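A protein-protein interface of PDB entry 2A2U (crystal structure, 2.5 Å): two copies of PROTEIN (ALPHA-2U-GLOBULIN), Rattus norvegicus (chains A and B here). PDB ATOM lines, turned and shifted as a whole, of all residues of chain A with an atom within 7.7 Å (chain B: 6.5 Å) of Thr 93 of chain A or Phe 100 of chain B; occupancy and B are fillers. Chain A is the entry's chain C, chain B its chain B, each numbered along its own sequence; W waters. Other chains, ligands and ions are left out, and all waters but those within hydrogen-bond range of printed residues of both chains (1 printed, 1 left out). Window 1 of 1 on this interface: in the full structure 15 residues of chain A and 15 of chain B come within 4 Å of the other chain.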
ATOM      1  N   ASN A  69      -1.660  20.331  -2.952  1.00  0.00           N
ATOM      2  CA  ASN A  69      -0.279  20.215  -3.426  1.00  0.00           C
ATOM      3  C   ASN A  69       0.656  19.667  -2.339  1.00  0.00           C
ATOM      4  O   ASN A  69       1.862  19.895  -2.380  1.00  0.00           O
ATOM      5  CB  ASN A  69       0.261  21.576  -3.914  1.00  0.00           C
ATOM      6  CG  ASN A  69      -0.578  22.192  -5.024  1.00  0.00           C
ATOM      7  OD1 ASN A  69      -0.798  21.581  -6.071  1.00  0.00           O
ATOM      8  ND2 ASN A  69      -1.020  23.428  -4.811  1.00  0.00           N
ATOM      9  N   VAL A  89       4.261  18.600   7.130  1.00  0.00           N
ATOM     10  CA  VAL A  89       3.674  18.771   5.812  1.00  0.00           C
ATOM     11  C   VAL A  89       4.772  18.565   4.772  1.00  0.00           C
ATOM     12  O   VAL A  89       5.876  19.077   4.912  1.00  0.00           O
ATOM     13  CB  VAL A  89       3.041  20.162   5.640  1.00  0.00           C
ATOM     14  CG1 VAL A  89       2.593  20.360   4.206  1.00  0.00           C
ATOM     15  CG2 VAL A  89       1.845  20.302   6.558  1.00  0.00           C
ATOM     16  N   ALA A  90       4.477  17.753   3.769  1.00  0.00           N
ATOM     17  CA  ALA A  90       5.414  17.459   2.699  1.00  0.00           C
ATOM     18  C   ALA A  90       4.832  18.067   1.433  1.00  0.00           C
ATOM     19  O   ALA A  90       3.675  17.848   1.126  1.00  0.00           O
ATOM     20  CB  ALA A  90       5.578  15.949   2.547  1.00  0.00           C
ATOM     21  N   TYR A  91       5.635  18.810   0.685  1.00  0.00           N
ATOM     22  CA  TYR A  91       5.158  19.456  -0.526  1.00  0.00           C
ATOM     23  C   TYR A  91       5.494  18.732  -1.800  1.00  0.00           C
ATOM     24  O   TYR A  91       6.561  18.148  -1.922  1.00  0.00           O
ATOM     25  CB  TYR A  91       5.740  20.835  -0.603  1.00  0.00           C
ATOM     26  CG  TYR A  91       5.412  21.632   0.601  1.00  0.00           C
ATOM     27  CD1 TYR A  91       4.134  22.149   0.780  1.00  0.00           C
ATOM     28  CD2 TYR A  91       6.366  21.864   1.571  1.00  0.00           C
ATOM     29  CE1 TYR A  91       3.811  22.886   1.904  1.00  0.00           C
ATOM     30  CE2 TYR A  91       6.063  22.593   2.696  1.00  0.00           C
ATOM     31  CZ  TYR A  91       4.781  23.102   2.860  1.00  0.00           C
ATOM     32  OH  TYR A  91       4.470  23.816   3.998  1.00  0.00           O
ATOM     33  N   LYS A  92       4.592  18.812  -2.764  1.00  0.00           N
ATOM     34  CA  LYS A  92       4.790  18.169  -4.053  1.00  0.00           C
ATOM     35  C   LYS A  92       5.774  19.016  -4.861  1.00  0.00           C
ATOM     36  O   LYS A  92       5.653  20.235  -4.894  1.00  0.00           O
ATOM     37  CB  LYS A  92       3.450  18.054  -4.781  1.00  0.00           C
ATOM     38  CG  LYS A  92       3.520  17.341  -6.105  1.00  0.00           C
ATOM     39  CD  LYS A  92       3.785  15.855  -5.962  1.00  0.00           C
ATOM     40  CE  LYS A  92       4.797  15.394  -6.996  1.00  0.00           C
ATOM     41  NZ  LYS A  92       4.397  15.756  -8.388  1.00  0.00           N
ATOM     42  N   THR A  93       6.771  18.380  -5.464  1.00  0.00           N
ATOM     43  CA  THR A  93       7.759  19.101  -6.258  1.00  0.00           C
ATOM     44  C   THR A  93       7.485  18.891  -7.743  1.00  0.00           C
ATOM     45  O   THR A  93       6.669  18.046  -8.114  1.00  0.00           O
ATOM     46  CB  THR A  93       9.199  18.637  -5.938  1.00  0.00           C
ATOM     47  OG1 THR A  93       9.474  17.402  -6.606  1.00  0.00           O
ATOM     48  CG2 THR A  93       9.380  18.442  -4.448  1.00  0.00           C
ATOM     49  N   PRO A  94       8.136  19.684  -8.614  1.00  0.00           N
ATOM     50  CA  PRO A  94       7.932  19.545 -10.058  1.00  0.00           C
ATOM     51  C   PRO A  94       8.438  18.248 -10.702  1.00  0.00           C
ATOM     52  O   PRO A  94       8.114  17.994 -11.857  1.00  0.00           O
ATOM     53  CB  PRO A  94       8.658  20.767 -10.626  1.00  0.00           C
ATOM     54  CG  PRO A  94       8.645  21.758  -9.508  1.00  0.00           C
ATOM     55  CD  PRO A  94       8.880  20.913  -8.302  1.00  0.00           C
ATOM     56  N   GLU A  95       9.230  17.443  -9.991  1.00  0.00           N
ATOM     57  CA  GLU A  95       9.746  16.181 -10.554  1.00  0.00           C
ATOM     58  C   GLU A  95       8.863  14.968 -10.186  1.00  0.00           C
ATOM     59  O   GLU A  95       8.751  14.612  -9.017  1.00  0.00           O
ATOM     60  CB  GLU A  95      11.202  15.932 -10.134  1.00  0.00           C
ATOM     61  CG  GLU A  95      11.880  17.016  -9.274  1.00  0.00           C
ATOM     62  CD  GLU A  95      12.202  18.309 -10.026  1.00  0.00           C
ATOM     63  OE1 GLU A  95      12.863  18.266 -11.087  1.00  0.00           O
ATOM     64  OE2 GLU A  95      11.798  19.380  -9.535  1.00  0.00           O
ATOM     65  N   ASP A  96       8.326  14.292 -11.202  1.00  0.00           N
ATOM     66  CA  ASP A  96       7.397  13.156 -11.062  1.00  0.00           C
ATOM     67  C   ASP A  96       7.385  12.266  -9.824  1.00  0.00           C
ATOM     68  O   ASP A  96       8.227  11.379  -9.627  1.00  0.00           O
ATOM     69  CB  ASP A  96       7.391  12.316 -12.360  1.00  0.00           C
ATOM     70  CG  ASP A  96       6.340  11.182 -12.364  1.00  0.00           C
ATOM     71  OD1 ASP A  96       5.116  11.431 -12.297  1.00  0.00           O
ATOM     72  OD2 ASP A  96       6.749  10.017 -12.511  1.00  0.00           O
ATOM     73  N   GLY A  97       6.379  12.529  -8.999  1.00  0.00           N
ATOM     74  CA  GLY A  97       6.160  11.763  -7.792  1.00  0.00           C
ATOM     75  C   GLY A  97       6.955  12.148  -6.575  1.00  0.00           C
ATOM     76  O   GLY A  97       6.753  11.556  -5.513  1.00  0.00           O
ATOM     77  N   GLU A  98       7.820  13.151  -6.707  1.00  0.00           N
ATOM     78  CA  GLU A  98       8.662  13.581  -5.594  1.00  0.00           C
ATOM     79  C   GLU A  98       8.037  14.594  -4.672  1.00  0.00           C
ATOM     80  O   GLU A  98       7.417  15.549  -5.112  1.00  0.00           O
ATOM     81  CB  GLU A  98       9.996  14.099  -6.101  1.00  0.00           C
ATOM     82  CG  GLU A  98      10.854  13.014  -6.705  1.00  0.00           C
ATOM     83  CD  GLU A  98      12.240  13.476  -7.066  1.00  0.00           C
ATOM     84  OE1 GLU A  98      12.656  14.561  -6.612  1.00  0.00           O
ATOM     85  OE2 GLU A  98      12.921  12.746  -7.812  1.00  0.00           O
ATOM     86  N   TYR A  99       8.197  14.345  -3.380  1.00  0.00           N
ATOM     87  CA  TYR A  99       7.686  15.218  -2.343  1.00  0.00           C
ATOM     88  C   TYR A  99       8.886  15.663  -1.525  1.00  0.00           C
ATOM     89  O   TYR A  99       9.885  14.947  -1.452  1.00  0.00           O
ATOM     90  CB  TYR A  99       6.721  14.455  -1.439  1.00  0.00           C
ATOM     91  CG  TYR A  99       5.368  14.215  -2.047  1.00  0.00           C
ATOM     92  CD1 TYR A  99       5.125  13.100  -2.847  1.00  0.00           C
ATOM     93  CD2 TYR A  99       4.331  15.106  -1.825  1.00  0.00           C
ATOM     94  CE1 TYR A  99       3.872  12.899  -3.434  1.00  0.00           C
ATOM     95  CE2 TYR A  99       3.086  14.919  -2.399  1.00  0.00           C
ATOM     96  CZ  TYR A  99       2.854  13.817  -3.198  1.00  0.00           C
ATOM     97  OH  TYR A  99       1.611  13.687  -3.796  1.00  0.00           O
ATOM     98  N   PHE A 100       8.803  16.854  -0.940  1.00  0.00           N
ATOM     99  CA  PHE A 100       9.878  17.363  -0.101  1.00  0.00           C
ATOM    100  C   PHE A 100       9.368  17.660   1.295  1.00  0.00           C
ATOM    101  O   PHE A 100       8.285  18.205   1.460  1.00  0.00           O
ATOM    102  CB  PHE A 100      10.486  18.649  -0.671  1.00  0.00           C
ATOM    103  CG  PHE A 100      11.544  19.262   0.233  1.00  0.00           C
ATOM    104  CD1 PHE A 100      12.875  18.857   0.144  1.00  0.00           C
ATOM    105  CD2 PHE A 100      11.190  20.178   1.224  1.00  0.00           C
ATOM    106  CE1 PHE A 100      13.830  19.345   1.032  1.00  0.00           C
ATOM    107  CE2 PHE A 100      12.141  20.668   2.113  1.00  0.00           C
ATOM    108  CZ  PHE A 100      13.458  20.249   2.016  1.00  0.00           C
ATOM    109  N   VAL A 101      10.169  17.326   2.298  1.00  0.00           N
ATOM    110  CA  VAL A 101       9.815  17.599   3.681  1.00  0.00           C
ATOM    111  C   VAL A 101      11.113  17.847   4.441  1.00  0.00           C
ATOM    112  O   VAL A 101      12.116  17.158   4.234  1.00  0.00           O
ATOM    113  CB  VAL A 101       8.975  16.438   4.316  1.00  0.00           C
ATOM    114  CG1 VAL A 101       9.776  15.140   4.393  1.00  0.00           C
ATOM    115  CG2 VAL A 101       8.474  16.837   5.677  1.00  0.00           C
ATOM    116  N   GLU A 102      11.119  18.908   5.237  1.00  0.00           N
ATOM    117  CA  GLU A 102      12.285  19.247   6.024  1.00  0.00           C
ATOM    118  C   GLU A 102      12.141  18.541   7.359  1.00  0.00           C
ATOM    119  O   GLU A 102      11.210  18.801   8.113  1.00  0.00           O
ATOM    120  CB  GLU A 102      12.392  20.763   6.212  1.00  0.00           C
ATOM    121  CG  GLU A 102      13.719  21.236   6.812  1.00  0.00           C
ATOM    122  CD  GLU A 102      14.918  21.051   5.883  1.00  0.00           C
ATOM    123  OE1 GLU A 102      14.731  20.849   4.666  1.00  0.00           O
ATOM    124  OE2 GLU A 102      16.063  21.123   6.371  1.00  0.00           O
ATOM    125  N   ASN A 107      14.587  16.174   2.902  1.00  0.00           N
ATOM    126  CA  ASN A 107      14.121  14.863   2.470  1.00  0.00           C
ATOM    127  C   ASN A 107      13.339  14.869   1.177  1.00  0.00           C
ATOM    128  O   ASN A 107      12.467  15.701   0.969  1.00  0.00           O
ATOM    129  CB  ASN A 107      13.225  14.237   3.539  1.00  0.00           C
ATOM    130  CG  ASN A 107      13.910  14.094   4.868  1.00  0.00           C
ATOM    131  OD1 ASN A 107      14.749  13.216   5.053  1.00  0.00           O
ATOM    132  ND2 ASN A 107      13.524  14.934   5.826  1.00  0.00           N
ATOM    133  N   THR A 108      13.625  13.888   0.338  1.00  0.00           N
ATOM    134  CA  THR A 108      12.923  13.714  -0.917  1.00  0.00           C
ATOM    135  C   THR A 108      12.376  12.294  -0.885  1.00  0.00           C
ATOM    136  O   THR A 108      13.124  11.341  -0.661  1.00  0.00           O
ATOM    137  CB  THR A 108      13.866  13.910  -2.108  1.00  0.00           C
ATOM    138  OG1 THR A 108      13.986  15.311  -2.384  1.00  0.00           O
ATOM    139  CG2 THR A 108      13.348  13.212  -3.340  1.00  0.00           C
ATOM    140  N   PHE A 109      11.063  12.154  -1.028  1.00  0.00           N
ATOM    141  CA  PHE A 109      10.462  10.827  -1.017  1.00  0.00           C
ATOM    142  C   PHE A 109       9.441  10.593  -2.108  1.00  0.00           C
ATOM    143  O   PHE A 109       8.928  11.536  -2.698  1.00  0.00           O
ATOM    144  CB  PHE A 109       9.862  10.495   0.348  1.00  0.00           C
ATOM    145  CG  PHE A 109       8.671  11.321   0.711  1.00  0.00           C
ATOM    146  CD1 PHE A 109       7.393  10.944   0.308  1.00  0.00           C
ATOM    147  CD2 PHE A 109       8.817  12.442   1.505  1.00  0.00           C
ATOM    148  CE1 PHE A 109       6.274  11.678   0.685  1.00  0.00           C
ATOM    149  CE2 PHE A 109       7.713  13.183   1.889  1.00  0.00           C
ATOM    150  CZ  PHE A 109       6.430  12.795   1.481  1.00  0.00           C
ATOM    151  N   VAL B  89      12.824  30.882   3.246  1.00  0.00           N
ATOM    152  CA  VAL B  89      13.936  29.965   3.427  1.00  0.00           C
ATOM    153  C   VAL B  89      13.778  28.825   2.424  1.00  0.00           C
ATOM    154  O   VAL B  89      12.691  28.286   2.247  1.00  0.00           O
ATOM    155  CB  VAL B  89      13.991  29.402   4.857  1.00  0.00           C
ATOM    156  CG1 VAL B  89      15.055  28.326   4.957  1.00  0.00           C
ATOM    157  CG2 VAL B  89      14.314  30.512   5.836  1.00  0.00           C
ATOM    158  N   ALA B  90      14.857  28.515   1.722  1.00  0.00           N
ATOM    159  CA  ALA B  90      14.867  27.452   0.732  1.00  0.00           C
ATOM    160  C   ALA B  90      15.786  26.367   1.270  1.00  0.00           C
ATOM    161  O   ALA B  90      16.896  26.652   1.676  1.00  0.00           O
ATOM    162  CB  ALA B  90      15.386  27.984  -0.602  1.00  0.00           C
ATOM    163  N   TYR B  91      15.335  25.121   1.256  1.00  0.00           N
ATOM    164  CA  TYR B  91      16.131  24.022   1.778  1.00  0.00           C
ATOM    165  C   TYR B  91      16.859  23.222   0.736  1.00  0.00           C
ATOM    166  O   TYR B  91      16.350  23.007  -0.355  1.00  0.00           O
ATOM    167  CB  TYR B  91      15.234  23.094   2.540  1.00  0.00           C
ATOM    168  CG  TYR B  91      14.511  23.801   3.622  1.00  0.00           C
ATOM    169  CD1 TYR B  91      15.171  24.172   4.789  1.00  0.00           C
ATOM    170  CD2 TYR B  91      13.174  24.116   3.485  1.00  0.00           C
ATOM    171  CE1 TYR B  91      14.511  24.840   5.801  1.00  0.00           C
ATOM    172  CE2 TYR B  91      12.502  24.781   4.480  1.00  0.00           C
ATOM    173  CZ  TYR B  91      13.176  25.145   5.640  1.00  0.00           C
ATOM    174  OH  TYR B  91      12.507  25.832   6.631  1.00  0.00           O
ATOM    175  N   LYS B  92      18.040  22.745   1.095  1.00  0.00           N
ATOM    176  CA  LYS B  92      18.849  21.945   0.191  1.00  0.00           C
ATOM    177  C   LYS B  92      18.261  20.535   0.146  1.00  0.00           C
ATOM    178  O   LYS B  92      17.922  19.977   1.183  1.00  0.00           O
ATOM    179  CB  LYS B  92      20.295  21.911   0.691  1.00  0.00           C
ATOM    180  CG  LYS B  92      21.248  21.164  -0.206  1.00  0.00           C
ATOM    181  CD  LYS B  92      21.515  21.883  -1.512  1.00  0.00           C
ATOM    182  CE  LYS B  92      21.512  20.900  -2.671  1.00  0.00           C
ATOM    183  NZ  LYS B  92      22.455  19.764  -2.457  1.00  0.00           N
ATOM    184  N   THR B  93      18.092  19.986  -1.051  1.00  0.00           N
ATOM    185  CA  THR B  93      17.537  18.645  -1.197  1.00  0.00           C
ATOM    186  C   THR B  93      18.650  17.658  -1.533  1.00  0.00           C
ATOM    187  O   THR B  93      19.774  18.061  -1.833  1.00  0.00           O
ATOM    188  CB  THR B  93      16.459  18.589  -2.304  1.00  0.00           C
ATOM    189  OG1 THR B  93      17.081  18.537  -3.592  1.00  0.00           O
ATOM    190  CG2 THR B  93      15.562  19.806  -2.240  1.00  0.00           C
ATOM    191  N   GLU B  98      19.929  21.078  -6.094  1.00  0.00           N
ATOM    192  CA  GLU B  98      18.523  21.454  -5.978  1.00  0.00           C
ATOM    193  C   GLU B  98      18.097  21.943  -4.620  1.00  0.00           C
ATOM    194  O   GLU B  98      18.453  21.368  -3.603  1.00  0.00           O
ATOM    195  CB  GLU B  98      17.624  20.311  -6.419  1.00  0.00           C
ATOM    196  CG  GLU B  98      17.723  20.025  -7.897  1.00  0.00           C
ATOM    197  CD  GLU B  98      16.726  19.005  -8.380  1.00  0.00           C
ATOM    198  OE1 GLU B  98      15.765  18.702  -7.645  1.00  0.00           O
ATOM    199  OE2 GLU B  98      16.907  18.503  -9.505  1.00  0.00           O
ATOM    200  N   TYR B  99      17.347  23.036  -4.629  1.00  0.00           N
ATOM    201  CA  TYR B  99      16.826  23.641  -3.420  1.00  0.00           C
ATOM    202  C   TYR B  99      15.313  23.642  -3.558  1.00  0.00           C
ATOM    203  O   TYR B  99      14.792  23.669  -4.673  1.00  0.00           O
ATOM    204  CB  TYR B  99      17.316  25.081  -3.297  1.00  0.00           C
ATOM    205  CG  TYR B  99      18.749  25.207  -2.866  1.00  0.00           C
ATOM    206  CD1 TYR B  99      19.788  25.185  -3.795  1.00  0.00           C
ATOM    207  CD2 TYR B  99      19.069  25.346  -1.525  1.00  0.00           C
ATOM    208  CE1 TYR B  99      21.121  25.273  -3.383  1.00  0.00           C
ATOM    209  CE2 TYR B  99      20.384  25.435  -1.102  1.00  0.00           C
ATOM    210  CZ  TYR B  99      21.408  25.403  -2.028  1.00  0.00           C
ATOM    211  OH  TYR B  99      22.713  25.445  -1.567  1.00  0.00           O
ATOM    212  N   PHE B 100      14.610  23.576  -2.432  1.00  0.00           N
ATOM    213  CA  PHE B 100      13.154  23.611  -2.443  1.00  0.00           C
ATOM    214  C   PHE B 100      12.642  24.774  -1.619  1.00  0.00           C
ATOM    215  O   PHE B 100      13.155  25.048  -0.542  1.00  0.00           O
ATOM    216  CB  PHE B 100      12.549  22.322  -1.876  1.00  0.00           C
ATOM    217  CG  PHE B 100      11.033  22.364  -1.782  1.00  0.00           C
ATOM    218  CD1 PHE B 100      10.243  21.992  -2.867  1.00  0.00           C
ATOM    219  CD2 PHE B 100      10.404  22.854  -0.636  1.00  0.00           C
ATOM    220  CE1 PHE B 100       8.857  22.120  -2.818  1.00  0.00           C
ATOM    221  CE2 PHE B 100       9.021  22.982  -0.583  1.00  0.00           C
ATOM    222  CZ  PHE B 100       8.251  22.616  -1.675  1.00  0.00           C
ATOM    223  N   VAL B 101      11.608  25.440  -2.117  1.00  0.00           N
ATOM    224  CA  VAL B 101      10.997  26.547  -1.403  1.00  0.00           C
ATOM    225  C   VAL B 101       9.516  26.559  -1.765  1.00  0.00           C
ATOM    226  O   VAL B 101       9.140  26.349  -2.922  1.00  0.00           O
ATOM    227  CB  VAL B 101      11.691  27.914  -1.726  1.00  0.00           C
ATOM    228  CG1 VAL B 101      11.530  28.295  -3.196  1.00  0.00           C
ATOM    229  CG2 VAL B 101      11.155  29.000  -0.832  1.00  0.00           C
ATOM    230  N   GLU B 102       8.677  26.692  -0.746  1.00  0.00           N
ATOM    231  CA  GLU B 102       7.246  26.731  -0.957  1.00  0.00           C
ATOM    232  C   GLU B 102       6.865  28.186  -1.154  1.00  0.00           C
ATOM    233  O   GLU B 102       7.038  29.008  -0.261  1.00  0.00           O
ATOM    234  CB  GLU B 102       6.504  26.124   0.238  1.00  0.00           C
ATOM    235  CG  GLU B 102       5.008  25.890   0.005  1.00  0.00           C
ATOM    236  CD  GLU B 102       4.707  24.792  -1.013  1.00  0.00           C
ATOM    237  OE1 GLU B 102       5.600  23.983  -1.333  1.00  0.00           O
ATOM    238  OE2 GLU B 102       3.557  24.726  -1.490  1.00  0.00           O
ATOM    239  N   TYR B 103       6.408  28.513  -2.354  1.00  0.00           N
ATOM    240  CA  TYR B 103       6.001  29.875  -2.669  1.00  0.00           C
ATOM    241  C   TYR B 103       5.148  29.856  -3.919  1.00  0.00           C
ATOM    242  O   TYR B 103       5.667  29.664  -5.013  1.00  0.00           O
ATOM    243  CB  TYR B 103       7.220  30.774  -2.906  1.00  0.00           C
ATOM    244  CG  TYR B 103       6.830  32.184  -3.300  1.00  0.00           C
ATOM    245  CD1 TYR B 103       6.296  33.068  -2.356  1.00  0.00           C
ATOM    246  CD2 TYR B 103       6.971  32.633  -4.611  1.00  0.00           C
ATOM    247  CE1 TYR B 103       5.915  34.367  -2.703  1.00  0.00           C
ATOM    248  CE2 TYR B 103       6.589  33.937  -4.973  1.00  0.00           C
ATOM    249  CZ  TYR B 103       6.063  34.792  -4.012  1.00  0.00           C
ATOM    250  OH  TYR B 103       5.685  36.073  -4.357  1.00  0.00           O
ATOM    251  N   GLY B 105       3.182  27.642  -4.733  1.00  0.00           N
ATOM    252  CA  GLY B 105       3.349  26.279  -5.203  1.00  0.00           C
ATOM    253  C   GLY B 105       4.647  25.674  -4.693  1.00  0.00           C
ATOM    254  O   GLY B 105       5.278  26.217  -3.782  1.00  0.00           O
ATOM    255  N   GLY B 106       5.029  24.535  -5.258  1.00  0.00           N
ATOM    256  CA  GLY B 106       6.257  23.880  -4.854  1.00  0.00           C
ATOM    257  C   GLY B 106       7.311  24.267  -5.857  1.00  0.00           C
ATOM    258  O   GLY B 106       7.125  24.054  -7.052  1.00  0.00           O
ATOM    259  N   ASN B 107       8.411  24.837  -5.378  1.00  0.00           N
ATOM    260  CA  ASN B 107       9.480  25.283  -6.259  1.00  0.00           C
ATOM    261  C   ASN B 107      10.783  24.535  -6.098  1.00  0.00           C
ATOM    262  O   ASN B 107      11.242  24.297  -4.989  1.00  0.00           O
ATOM    263  CB  ASN B 107       9.778  26.765  -6.031  1.00  0.00           C
ATOM    264  CG  ASN B 107       8.578  27.644  -6.240  1.00  0.00           C
ATOM    265  OD1 ASN B 107       8.175  27.897  -7.372  1.00  0.00           O
ATOM    266  ND2 ASN B 107       8.019  28.155  -5.147  1.00  0.00           N
ATOM    267  N   THR B 108      11.401  24.222  -7.224  1.00  0.00           N
ATOM    268  CA  THR B 108      12.689  23.560  -7.243  1.00  0.00           C
ATOM    269  C   THR B 108      13.599  24.459  -8.067  1.00  0.00           C
ATOM    270  O   THR B 108      13.269  24.813  -9.199  1.00  0.00           O
ATOM    271  CB  THR B 108      12.583  22.166  -7.870  1.00  0.00           C
ATOM    272  OG1 THR B 108      12.135  21.238  -6.875  1.00  0.00           O
ATOM    273  CG2 THR B 108      13.914  21.702  -8.405  1.00  0.00           C
ATOM    274  N   PHE B 109      14.707  24.895  -7.477  1.00  0.00           N
ATOM    275  CA  PHE B 109      15.633  25.754  -8.202  1.00  0.00           C
ATOM    276  C   PHE B 109      17.088  25.370  -8.054  1.00  0.00           C
ATOM    277  O   PHE B 109      17.453  24.640  -7.139  1.00  0.00           O
ATOM    278  CB  PHE B 109      15.437  27.225  -7.837  1.00  0.00           C
ATOM    279  CG  PHE B 109      15.815  27.564  -6.433  1.00  0.00           C
ATOM    280  CD1 PHE B 109      17.128  27.891  -6.108  1.00  0.00           C
ATOM    281  CD2 PHE B 109      14.850  27.615  -5.444  1.00  0.00           C
ATOM    282  CE1 PHE B 109      17.479  28.259  -4.813  1.00  0.00           C
ATOM    283  CE2 PHE B 109      15.182  27.979  -4.152  1.00  0.00           C
ATOM    284  CZ  PHE B 109      16.507  28.310  -3.834  1.00  0.00           C
ATOM    285  N   PHE B 127       5.536  24.189  -9.417  1.00  0.00           N
ATOM    286  CA  PHE B 127       4.439  23.237  -9.534  1.00  0.00           C
ATOM    287  C   PHE B 127       3.270  23.692  -8.683  1.00  0.00           C
ATOM    288  O   PHE B 127       3.419  23.934  -7.487  1.00  0.00           O
ATOM    289  CB  PHE B 127       4.836  21.842  -9.092  1.00  0.00           C
ATOM    290  CG  PHE B 127       3.688  20.894  -9.044  1.00  0.00           C
ATOM    291  CD1 PHE B 127       3.307  20.185 -10.174  1.00  0.00           C
ATOM    292  CD2 PHE B 127       2.935  20.773  -7.883  1.00  0.00           C
ATOM    293  CE1 PHE B 127       2.190  19.375 -10.146  1.00  0.00           C
ATOM    294  CE2 PHE B 127       1.822  19.973  -7.843  1.00  0.00           C
ATOM    295  CZ  PHE B 127       1.442  19.271  -8.975  1.00  0.00           C
ATOM    296  N   THR B 132       3.020  23.275 -14.190  1.00  0.00           N
ATOM    297  CA  THR B 132       4.399  23.678 -13.962  1.00  0.00           C
ATOM    298  C   THR B 132       4.805  24.786 -14.925  1.00  0.00           C
ATOM    299  O   THR B 132       4.120  25.050 -15.911  1.00  0.00           O
ATOM    300  CB  THR B 132       5.387  22.521 -14.184  1.00  0.00           C
ATOM    301  OG1 THR B 132       5.353  22.124 -15.559  1.00  0.00           O
ATOM    302  CG2 THR B 132       5.051  21.335 -13.306  1.00  0.00           C
HETATM  303  O   HOH W   1      17.851  20.777   4.131  1.00  0.00           O
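The side-chain carboxylate of Glu 95 of chain A lies within hydrogen-bond range of the side-chain hydroxyl of Thr 108 of chain B (3.3 Å).
The backbone carbonyl oxygen (O) of Tyr 91 of chain B lies within hydrogen-bond range of the backbone NH (N) of Phe 100 of chain B (2.8 Å). N of Thr 93 of chain B is in hydrogen-bond range of O of Glu 98 of chain B (2.9 Å). N of Gly 106 of chain B is in hydrogen-bond range of O of Phe 127 of chain B, at 2.8 Å. O of Asn 69 of chain A lies within hydrogen-bond range of N of Lys 92 of chain A (3.0 Å). The backbone carbonyl oxygen of Tyr 91 of chain A sits at hydrogen-bond distance from the backbone NH of Phe 100 of chain A (2.8 Å). OG1 of Thr 93 of chain A sits close to N of Glu 95 of chain A (3.4 Å).
Among the printed residues, merely in contact across the chains: Asn 69 of chain A with Phe 127 of chain B (3.5 Å), Tyr 91 of chain A with Phe 100 of chain B (3.3 Å), Tyr 91 of chain A with Glu 102 of chain B (3.1 Å), Lys 92 of chain A with Gly 106 of chain B (3.7 Å), Lys 92 of chain A with Phe 127 of chain B (3.6 Å), Thr 93 of chain A with Phe 100 of chain B (3.98 Å), Pro 94 of chain A with Gly 106 of chain B (3.7 Å), Pro 94 of chain A with Thr 108 of chain B (3.6 Å), Pro 94 of chain A with Phe 127 of chain B (3.8 Å), Phe 100 of chain A with Tyr 91 of chain B (3.4 Å), Phe 100 of chain A with Thr 93 of chain B (3.7 Å), Phe 100 of chain A with Phe 100 of chain B (3.4 Å) and Glu 102 of chain A with Tyr 91 of chain B (3.1 Å).
Printed residues of chain B within 4 Å of Thr 93 of chain A: Phe 100 (3.98 Å). Printed residues of chain A within 4 Å of Phe 100 of chain B: Tyr 91, Thr 93 and Phe 100. Of the printed residues of chain A, Thr 93 of chain B touches Phe 100. Of the printed residues of chain A, Phe 127 of chain B touches Asn 69 (3.5 Å), Lys 92 (3.6 Å) and Pro 94 (3.8 Å). Printed residues of chain B within 4 Å of Glu 102 of chain A: Tyr 91. Printed residues of chain A within 4 Å of Tyr 91 of chain B: Phe 100 and Glu 102. Phe 109 of chain A touches none of the printed residues of chain B. Glu 98 of chain B touches none of the printed residues of chain A. The nearest printed residue of chain B that does not touch Thr 93 of chain A is Thr 108 of chain B (4.03 Å). The nearest printed residue of chain A that does not touch Phe 100 of chain B is Lys 92 of chain A (4.3 Å).
Printed residues of chain A that touch a printed residue of chain B: Asn 69, Tyr 91, Lys 92, Thr 93, Pro 94, Glu 95, Phe 100 and Glu 102. Of the 18 printed residues of chain B, 7 touch a printed residue of chain A. Hydrophobic or aromatic side chains of chain B that line the printed part of chain A: Tyr 91, Phe 100 and Phe 127. Among the printed residues, 14 pairs touch across the chains.
Tyr 91 of chain A touches Phe 100 of chain B, and with the chains exchanged Phe 100 of chain A touches Tyr 91 of chain B. Tyr 91 of chain A touches Glu 102 of chain B, and with the chains exchanged Glu 102 of chain A touches Tyr 91 of chain B. Thr 93 of chain A touches Phe 100 of chain B, and with the chains exchanged Phe 100 of chain A touches Thr 93 of chain B. Phe 100 of chain A touches its own counterpart, Phe 100 of chain B. 13 positions are printed for both chains. Of the 14 pairs that touch across the chains among the printed residues, 7 have their exchanged pair printed and touching as well.
Water W1 bridges the side-chain carboxylate (OE2) of Glu 102 of chain A and the backbone carbonyl oxygen (O) of Lys 92 of chain B.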
